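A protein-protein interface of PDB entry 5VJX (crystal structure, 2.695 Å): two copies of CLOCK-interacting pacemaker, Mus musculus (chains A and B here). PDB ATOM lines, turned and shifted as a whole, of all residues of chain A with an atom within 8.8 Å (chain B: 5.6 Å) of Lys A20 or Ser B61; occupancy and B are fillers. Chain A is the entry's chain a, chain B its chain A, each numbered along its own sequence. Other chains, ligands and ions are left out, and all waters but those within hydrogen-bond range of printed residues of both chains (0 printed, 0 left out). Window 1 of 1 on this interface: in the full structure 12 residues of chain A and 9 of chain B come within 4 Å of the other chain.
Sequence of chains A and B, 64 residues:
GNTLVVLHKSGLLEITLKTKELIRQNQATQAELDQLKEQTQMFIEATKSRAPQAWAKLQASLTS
Among the printed residues, merely in contact across the chains: Leu A13 with Leu B62 (3.6 Å), Thr A16 with Leu B62 (3.1 Å), Leu A17 with Leu B62 (3.97 Å) and Arg A24 with Gln B35 (3.0 Å).
Lys A20 touches one residue of chain B.
Of chain A, only Lys A20 (2.4 Å) comes within 4 Å of Ser B61.
No residue of chain A comes within 4 Å of Ala B60.
Printed residues of chain B within 4 Å of Thr A16: Leu B62.
Of the printed residues of chain A, Leu B62 touches Leu A13 (3.6 Å), Thr A16 (3.1 Å) and Leu A17 (3.97 Å).
Of the printed residues of chain B, Leu A17 touches Leu B62.
Of the printed residues of chain B, Leu A13 touches Leu B62.
Hydrophobic or aromatic side chains of chain A within 4 Å of the printed part of chain B: Leu A13 and Leu A17.
Hydrophobic or aromatic side chains of chain B within 4 Å of the printed part of chain A: Leu B62.
Among the printed residues, no Asp or Glu carboxylate lies within 4 Å of a Lys or Arg side-chain nitrogen of the other chain.
O of Leu A12 sits at hydrogen-bond distance from OG1 of Thr A16, 2.5 Å away.
O of Leu A7 sits at hydrogen-bond distance from N of Leu A13, 3.2 Å away.
OE2 of Glu A21 lies within salt-bridge range of NH2 of Arg A24 (2.9 Å).
No position is printed for both chains.
O of Ser B61 is in hydrogen-bond range of NZ of Lys A20.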
ATOM      1  N   LEU A   7      30.948  11.672  24.619  1.00  0.00           N
ATOM      2  CA  LEU A   7      31.051  11.637  23.165  1.00  0.00           C
ATOM      3  C   LEU A   7      31.354  12.989  22.570  1.00  0.00           C
ATOM      4  O   LEU A   7      32.193  13.100  21.689  1.00  0.00           O
ATOM      5  CB  LEU A   7      29.766  11.123  22.524  1.00  0.00           C
ATOM      6  CG  LEU A   7      29.516   9.644  22.337  1.00  0.00           C
ATOM      7  CD1 LEU A   7      28.132   9.440  21.787  1.00  0.00           C
ATOM      8  CD2 LEU A   7      30.503   9.226  21.302  1.00  0.00           C
ATOM      9  N   LEU A  12      34.282  12.378  19.505  1.00  0.00           N
ATOM     10  CA  LEU A  12      33.976  11.230  18.664  1.00  0.00           C
ATOM     11  C   LEU A  12      32.594  11.424  18.045  1.00  0.00           C
ATOM     12  O   LEU A  12      32.192  10.704  17.134  1.00  0.00           O
ATOM     13  CB  LEU A  12      33.998   9.937  19.474  1.00  0.00           C
ATOM     14  CG  LEU A  12      35.345   9.408  19.944  1.00  0.00           C
ATOM     15  CD1 LEU A  12      35.167   8.149  20.756  1.00  0.00           C
ATOM     16  CD2 LEU A  12      36.180   9.121  18.738  1.00  0.00           C
ATOM     17  N   LEU A  13      31.881  12.433  18.525  1.00  0.00           N
ATOM     18  CA  LEU A  13      30.557  12.714  18.023  1.00  0.00           C
ATOM     19  C   LEU A  13      30.687  13.251  16.621  1.00  0.00           C
ATOM     20  O   LEU A  13      30.117  12.716  15.670  1.00  0.00           O
ATOM     21  CB  LEU A  13      29.838  13.715  18.925  1.00  0.00           C
ATOM     22  CG  LEU A  13      28.370  13.982  18.599  1.00  0.00           C
ATOM     23  CD1 LEU A  13      27.599  12.693  18.675  1.00  0.00           C
ATOM     24  CD2 LEU A  13      27.794  14.997  19.556  1.00  0.00           C
ATOM     25  N   GLU A  14      31.489  14.300  16.516  1.00  0.00           N
ATOM     26  CA  GLU A  14      31.784  14.971  15.262  1.00  0.00           C
ATOM     27  C   GLU A  14      32.331  13.996  14.240  1.00  0.00           C
ATOM     28  O   GLU A  14      31.940  14.008  13.076  1.00  0.00           O
ATOM     29  CB  GLU A  14      32.759  16.116  15.517  1.00  0.00           C
ATOM     30  CG  GLU A  14      33.130  16.932  14.308  1.00  0.00           C
ATOM     31  CD  GLU A  14      33.941  18.149  14.685  1.00  0.00           C
ATOM     32  OE1 GLU A  14      34.117  18.392  15.896  1.00  0.00           O
ATOM     33  OE2 GLU A  14      34.405  18.861  13.775  1.00  0.00           O
ATOM     34  N   ILE A  15      33.248  13.153  14.687  1.00  0.00           N
ATOM     35  CA  ILE A  15      33.841  12.147  13.834  1.00  0.00           C
ATOM     36  C   ILE A  15      32.804  11.150  13.340  1.00  0.00           C
ATOM     37  O   ILE A  15      32.802  10.791  12.169  1.00  0.00           O
ATOM     38  CB  ILE A  15      34.933  11.384  14.576  1.00  0.00           C
ATOM     39  CG1 ILE A  15      36.091  12.305  14.912  1.00  0.00           C
ATOM     40  CG2 ILE A  15      35.405  10.216  13.756  1.00  0.00           C
ATOM     41  CD1 ILE A  15      37.085  11.674  15.805  1.00  0.00           C
ATOM     42  N   THR A  16      31.915  10.710  14.230  1.00  0.00           N
ATOM     43  CA  THR A  16      30.887   9.743  13.852  1.00  0.00           C
ATOM     44  C   THR A  16      29.961  10.301  12.801  1.00  0.00           C
ATOM     45  O   THR A  16      29.606   9.628  11.833  1.00  0.00           O
ATOM     46  CB  THR A  16      30.032   9.320  15.041  1.00  0.00           C
ATOM     47  OG1 THR A  16      30.868   8.809  16.077  1.00  0.00           O
ATOM     48  CG2 THR A  16      29.074   8.239  14.618  1.00  0.00           C
ATOM     49  N   LEU A  17      29.571  11.545  13.002  1.00  0.00           N
ATOM     50  CA  LEU A  17      28.671  12.216  12.091  1.00  0.00           C
ATOM     51  C   LEU A  17      29.276  12.502  10.723  1.00  0.00           C
ATOM     52  O   LEU A  17      28.659  12.225   9.690  1.00  0.00           O
ATOM     53  CB  LEU A  17      28.219  13.484  12.753  1.00  0.00           C
ATOM     54  CG  LEU A  17      27.320  13.217  13.956  1.00  0.00           C
ATOM     55  CD1 LEU A  17      27.497  14.292  14.990  1.00  0.00           C
ATOM     56  CD2 LEU A  17      25.871  13.153  13.526  1.00  0.00           C
ATOM     57  N   LYS A  18      30.483  13.064  10.716  1.00  0.00           N
ATOM     58  CA  LYS A  18      31.201  13.309   9.466  1.00  0.00           C
ATOM     59  C   LYS A  18      31.459  11.993   8.735  1.00  0.00           C
ATOM     60  O   LYS A  18      31.435  11.952   7.517  1.00  0.00           O
ATOM     61  CB  LYS A  18      32.502  14.088   9.695  1.00  0.00           C
ATOM     62  CG  LYS A  18      32.245  15.524  10.134  1.00  0.00           C
ATOM     63  CD  LYS A  18      33.487  16.384  10.298  1.00  0.00           C
ATOM     64  CE  LYS A  18      34.113  16.656   8.935  1.00  0.00           C
ATOM     65  NZ  LYS A  18      33.234  17.464   8.034  1.00  0.00           N
ATOM     66  N   THR A  19      31.722  10.923   9.485  1.00  0.00           N
ATOM     67  CA  THR A  19      31.962   9.601   8.909  1.00  0.00           C
ATOM     68  C   THR A  19      30.690   9.006   8.287  1.00  0.00           C
ATOM     69  O   THR A  19      30.737   8.449   7.204  1.00  0.00           O
ATOM     70  CB  THR A  19      32.530   8.628   9.959  1.00  0.00           C
ATOM     71  OG1 THR A  19      33.823   9.071  10.372  1.00  0.00           O
ATOM     72  CG2 THR A  19      32.670   7.245   9.391  1.00  0.00           C
ATOM     73  N   LYS A  20      29.551   9.118   8.963  1.00  0.00           N
ATOM     74  CA  LYS A  20      28.300   8.637   8.377  1.00  0.00           C
ATOM     75  C   LYS A  20      27.926   9.438   7.140  1.00  0.00           C
ATOM     76  O   LYS A  20      27.378   8.898   6.183  1.00  0.00           O
ATOM     77  CB  LYS A  20      27.159   8.664   9.389  1.00  0.00           C
ATOM     78  CG  LYS A  20      27.212   7.509  10.383  1.00  0.00           C
ATOM     79  CD  LYS A  20      25.915   7.369  11.162  1.00  0.00           C
ATOM     80  CE  LYS A  20      25.689   5.915  11.559  1.00  0.00           C
ATOM     81  NZ  LYS A  20      24.409   5.728  12.290  1.00  0.00           N
ATOM     82  N   GLU A  21      28.211  10.734   7.176  1.00  0.00           N
ATOM     83  CA  GLU A  21      27.963  11.617   6.037  1.00  0.00           C
ATOM     84  C   GLU A  21      28.855  11.276   4.828  1.00  0.00           C
ATOM     85  O   GLU A  21      28.410  11.304   3.678  1.00  0.00           O
ATOM     86  CB  GLU A  21      28.179  13.073   6.454  1.00  0.00           C
ATOM     87  CG  GLU A  21      27.766  14.106   5.417  1.00  0.00           C
ATOM     88  CD  GLU A  21      26.285  14.061   5.097  1.00  0.00           C
ATOM     89  OE1 GLU A  21      25.515  13.438   5.857  1.00  0.00           O
ATOM     90  OE2 GLU A  21      25.888  14.663   4.080  1.00  0.00           O
ATOM     91  N   LEU A  22      30.128  11.000   5.098  1.00  0.00           N
ATOM     92  CA  LEU A  22      31.077  10.598   4.065  1.00  0.00           C
ATOM     93  C   LEU A  22      30.732   9.251   3.461  1.00  0.00           C
ATOM     94  O   LEU A  22      30.922   9.036   2.267  1.00  0.00           O
ATOM     95  CB  LEU A  22      32.488  10.549   4.623  1.00  0.00           C
ATOM     96  CG  LEU A  22      33.563  10.142   3.619  1.00  0.00           C
ATOM     97  CD1 LEU A  22      33.562  11.036   2.408  1.00  0.00           C
ATOM     98  CD2 LEU A  22      34.915  10.132   4.280  1.00  0.00           C
ATOM     99  N   ILE A  23      30.253   8.339   4.302  1.00  0.00           N
ATOM    100  CA  ILE A  23      29.752   7.050   3.851  1.00  0.00           C
ATOM    101  C   ILE A  23      28.548   7.227   2.937  1.00  0.00           C
ATOM    102  O   ILE A  23      28.434   6.585   1.896  1.00  0.00           O
ATOM    103  CB  ILE A  23      29.367   6.167   5.034  1.00  0.00           C
ATOM    104  CG1 ILE A  23      30.624   5.643   5.717  1.00  0.00           C
ATOM    105  CG2 ILE A  23      28.533   4.998   4.570  1.00  0.00           C
ATOM    106  CD1 ILE A  23      30.390   5.031   7.046  1.00  0.00           C
ATOM    107  N   ARG A  24      27.658   8.119   3.334  1.00  0.00           N
ATOM    108  CA  ARG A  24      26.476   8.424   2.554  1.00  0.00           C
ATOM    109  C   ARG A  24      26.873   8.937   1.167  1.00  0.00           C
ATOM    110  O   ARG A  24      26.397   8.453   0.131  1.00  0.00           O
ATOM    111  CB  ARG A  24      25.640   9.464   3.287  1.00  0.00           C
ATOM    112  CG  ARG A  24      24.248   9.633   2.760  1.00  0.00           C
ATOM    113  CD  ARG A  24      23.647  10.951   3.209  1.00  0.00           C
ATOM    114  NE  ARG A  24      24.494  12.082   2.851  1.00  0.00           N
ATOM    115  CZ  ARG A  24      24.574  12.581   1.624  1.00  0.00           C
ATOM    116  NH1 ARG A  24      23.881  12.036   0.640  1.00  0.00           N
ATOM    117  NH2 ARG A  24      25.358  13.614   1.375  1.00  0.00           N
ATOM    118  N   GLN A  25      27.754   9.927   1.163  1.00  0.00           N
ATOM    119  CA  GLN A  25      28.233  10.530  -0.071  1.00  0.00           C
ATOM    120  C   GLN A  25      28.905   9.495  -0.966  1.00  0.00           C
ATOM    121  O   GLN A  25      28.701   9.473  -2.178  1.00  0.00           O
ATOM    122  CB  GLN A  25      29.189  11.679   0.246  1.00  0.00           C
ATOM    123  CG  GLN A  25      28.481  12.898   0.810  1.00  0.00           C
ATOM    124  CD  GLN A  25      29.415  14.056   1.103  1.00  0.00           C
ATOM    125  OE1 GLN A  25      30.639  13.905   1.087  1.00  0.00           O
ATOM    126  NE2 GLN A  25      28.835  15.225   1.383  1.00  0.00           N
ATOM    127  N   ASN A  26      29.706   8.634  -0.356  1.00  0.00           N
ATOM    128  CA  ASN A  26      30.400   7.588  -1.086  1.00  0.00           C
ATOM    129  C   ASN A  26      29.453   6.575  -1.710  1.00  0.00           C
ATOM    130  O   ASN A  26      29.709   6.070  -2.798  1.00  0.00           O
ATOM    131  CB  ASN A  26      31.373   6.878  -0.162  1.00  0.00           C
ATOM    132  CG  ASN A  26      32.242   5.899  -0.888  1.00  0.00           C
ATOM    133  OD1 ASN A  26      32.797   6.207  -1.935  1.00  0.00           O
ATOM    134  ND2 ASN A  26      32.359   4.695  -0.338  1.00  0.00           N
ATOM    135  N   GLN A  27      28.360   6.272  -1.023  1.00  0.00           N
ATOM    136  CA  GLN A  27      27.357   5.386  -1.599  1.00  0.00           C
ATOM    137  C   GLN A  27      26.661   6.043  -2.779  1.00  0.00           C
ATOM    138  O   GLN A  27      26.359   5.383  -3.774  1.00  0.00           O
ATOM    139  CB  GLN A  27      26.327   4.969  -0.561  1.00  0.00           C
ATOM    140  CG  GLN A  27      26.316   3.480  -0.314  1.00  0.00           C
ATOM    141  CD  GLN A  27      26.299   2.673  -1.599  1.00  0.00           C
ATOM    142  OE1 GLN A  27      27.195   1.867  -1.845  1.00  0.00           O
ATOM    143  NE2 GLN A  27      25.274   2.878  -2.420  1.00  0.00           N
ATOM    144  N   GLN B  35      16.784  11.447   4.050  1.00  0.00           N
ATOM    145  CA  GLN B  35      17.616  11.040   5.176  1.00  0.00           C
ATOM    146  C   GLN B  35      17.762  12.156   6.205  1.00  0.00           C
ATOM    147  O   GLN B  35      17.619  11.928   7.410  1.00  0.00           O
ATOM    148  CB  GLN B  35      18.979  10.587   4.679  1.00  0.00           C
ATOM    149  CG  GLN B  35      19.815   9.903   5.723  1.00  0.00           C
ATOM    150  CD  GLN B  35      21.028   9.243   5.117  1.00  0.00           C
ATOM    151  OE1 GLN B  35      21.220   9.285   3.905  1.00  0.00           O
ATOM    152  NE2 GLN B  35      21.857   8.629   5.953  1.00  0.00           N
ATOM    153  N   MET B  42      14.162  12.845  14.291  1.00  0.00           N
ATOM    154  CA  MET B  42      14.618  12.063  15.432  1.00  0.00           C
ATOM    155  C   MET B  42      15.394  12.926  16.420  1.00  0.00           C
ATOM    156  O   MET B  42      15.286  12.750  17.631  1.00  0.00           O
ATOM    157  CB  MET B  42      15.468  10.884  14.961  1.00  0.00           C
ATOM    158  CG  MET B  42      16.261  10.230  16.071  1.00  0.00           C
ATOM    159  SD  MET B  42      17.179   8.626  15.488  1.00  0.00           S
ATOM    160  CE  MET B  42      17.329   9.055  13.597  1.00  0.00           C
ATOM    161  N   ALA B  56      17.141   7.015  23.368  1.00  0.00           N
ATOM    162  CA  ALA B  56      17.828   5.755  23.193  1.00  0.00           C
ATOM    163  C   ALA B  56      17.975   5.496  21.721  1.00  0.00           C
ATOM    164  O   ALA B  56      18.976   4.960  21.277  1.00  0.00           O
ATOM    165  CB  ALA B  56      17.073   4.630  23.869  1.00  0.00           C
ATOM    166  N   LYS B  57      16.941   5.853  20.977  1.00  0.00           N
ATOM    167  CA  LYS B  57      16.937   5.665  19.547  1.00  0.00           C
ATOM    168  C   LYS B  57      18.055   6.476  18.901  1.00  0.00           C
ATOM    169  O   LYS B  57      18.829   5.944  18.110  1.00  0.00           O
ATOM    170  CB  LYS B  57      15.576   6.075  18.982  1.00  0.00           C
ATOM    171  CG  LYS B  57      15.444   5.964  17.485  1.00  0.00           C
ATOM    172  CD  LYS B  57      14.074   6.437  17.019  1.00  0.00           C
ATOM    173  CE  LYS B  57      13.911   6.253  15.515  1.00  0.00           C
ATOM    174  NZ  LYS B  57      12.577   6.672  14.985  1.00  0.00           N
ATOM    175  N   LEU B  58      18.170   7.747  19.274  1.00  0.00           N
ATOM    176  CA  LEU B  58      19.193   8.607  18.689  1.00  0.00           C
ATOM    177  C   LEU B  58      20.581   8.120  19.064  1.00  0.00           C
ATOM    178  O   LEU B  58      21.463   7.988  18.210  1.00  0.00           O
ATOM    179  CB  LEU B  58      19.014  10.064  19.126  1.00  0.00           C
ATOM    180  CG  LEU B  58      20.107  11.013  18.620  1.00  0.00           C
ATOM    181  CD1 LEU B  58      20.022  11.123  17.113  1.00  0.00           C
ATOM    182  CD2 LEU B  58      20.048  12.392  19.257  1.00  0.00           C
ATOM    183  N   GLN B  59      20.765   7.825  20.344  1.00  0.00           N
ATOM    184  CA  GLN B  59      22.067   7.384  20.811  1.00  0.00           C
ATOM    185  C   GLN B  59      22.450   6.069  20.138  1.00  0.00           C
ATOM    186  O   GLN B  59      23.615   5.849  19.829  1.00  0.00           O
ATOM    187  CB  GLN B  59      22.070   7.280  22.335  1.00  0.00           C
ATOM    188  CG  GLN B  59      23.417   6.959  22.958  1.00  0.00           C
ATOM    189  CD  GLN B  59      23.312   6.763  24.457  1.00  0.00           C
ATOM    190  OE1 GLN B  59      22.299   7.107  25.064  1.00  0.00           O
ATOM    191  NE2 GLN B  59      24.365   6.235  25.066  1.00  0.00           N
ATOM    192  N   ALA B  60      21.470   5.199  19.918  1.00  0.00           N
ATOM    193  CA  ALA B  60      21.686   3.954  19.189  1.00  0.00           C
ATOM    194  C   ALA B  60      22.042   4.243  17.739  1.00  0.00           C
ATOM    195  O   ALA B  60      22.791   3.495  17.118  1.00  0.00           O
ATOM    196  CB  ALA B  60      20.461   3.058  19.261  1.00  0.00           C
ATOM    197  N   SER B  61      21.483   5.319  17.197  1.00  0.00           N
ATOM    198  CA  SER B  61      21.758   5.695  15.819  1.00  0.00           C
ATOM    199  C   SER B  61      23.183   6.200  15.651  1.00  0.00           C
ATOM    200  O   SER B  61      23.769   6.076  14.580  1.00  0.00           O
ATOM    201  CB  SER B  61      20.770   6.755  15.345  1.00  0.00           C
ATOM    202  OG  SER B  61      21.076   7.172  14.028  1.00  0.00           O
ATOM    203  N   LEU B  62      23.725   6.818  16.691  1.00  0.00           N
ATOM    204  CA  LEU B  62      25.092   7.328  16.612  1.00  0.00           C
ATOM    205  C   LEU B  62      26.174   6.266  16.830  1.00  0.00           C
ATOM    206  O   LEU B  62      27.323   6.468  16.462  1.00  0.00           O
ATOM    207  CB  LEU B  62      25.283   8.465  17.604  1.00  0.00           C
ATOM    208  CG  LEU B  62      24.398   9.662  17.276  1.00  0.00           C
ATOM    209  CD1 LEU B  62      24.585  10.738  18.318  1.00  0.00           C
ATOM    210  CD2 LEU B  62      24.698  10.180  15.883  1.00  0.00           C
ATOM    211  N   THR B  63      25.814   5.143  17.438  1.00  0.00           N
ATOM    212  CA  THR B  63      26.802   4.124  17.776  1.00  0.00           C
ATOM    213  C   THR B  63      26.711   2.907  16.863  1.00  0.00           C
ATOM    214  O   THR B  63      26.563   3.042  15.653  1.00  0.00           O
ATOM    215  CB  THR B  63      26.653   3.662  19.231  1.00  0.00           C
ATOM    216  OG1 THR B  63      26.791   4.788  20.105  1.00  0.00           O
ATOM    217  CG2 THR B  63      27.716   2.632  19.574  1.00  0.00           C
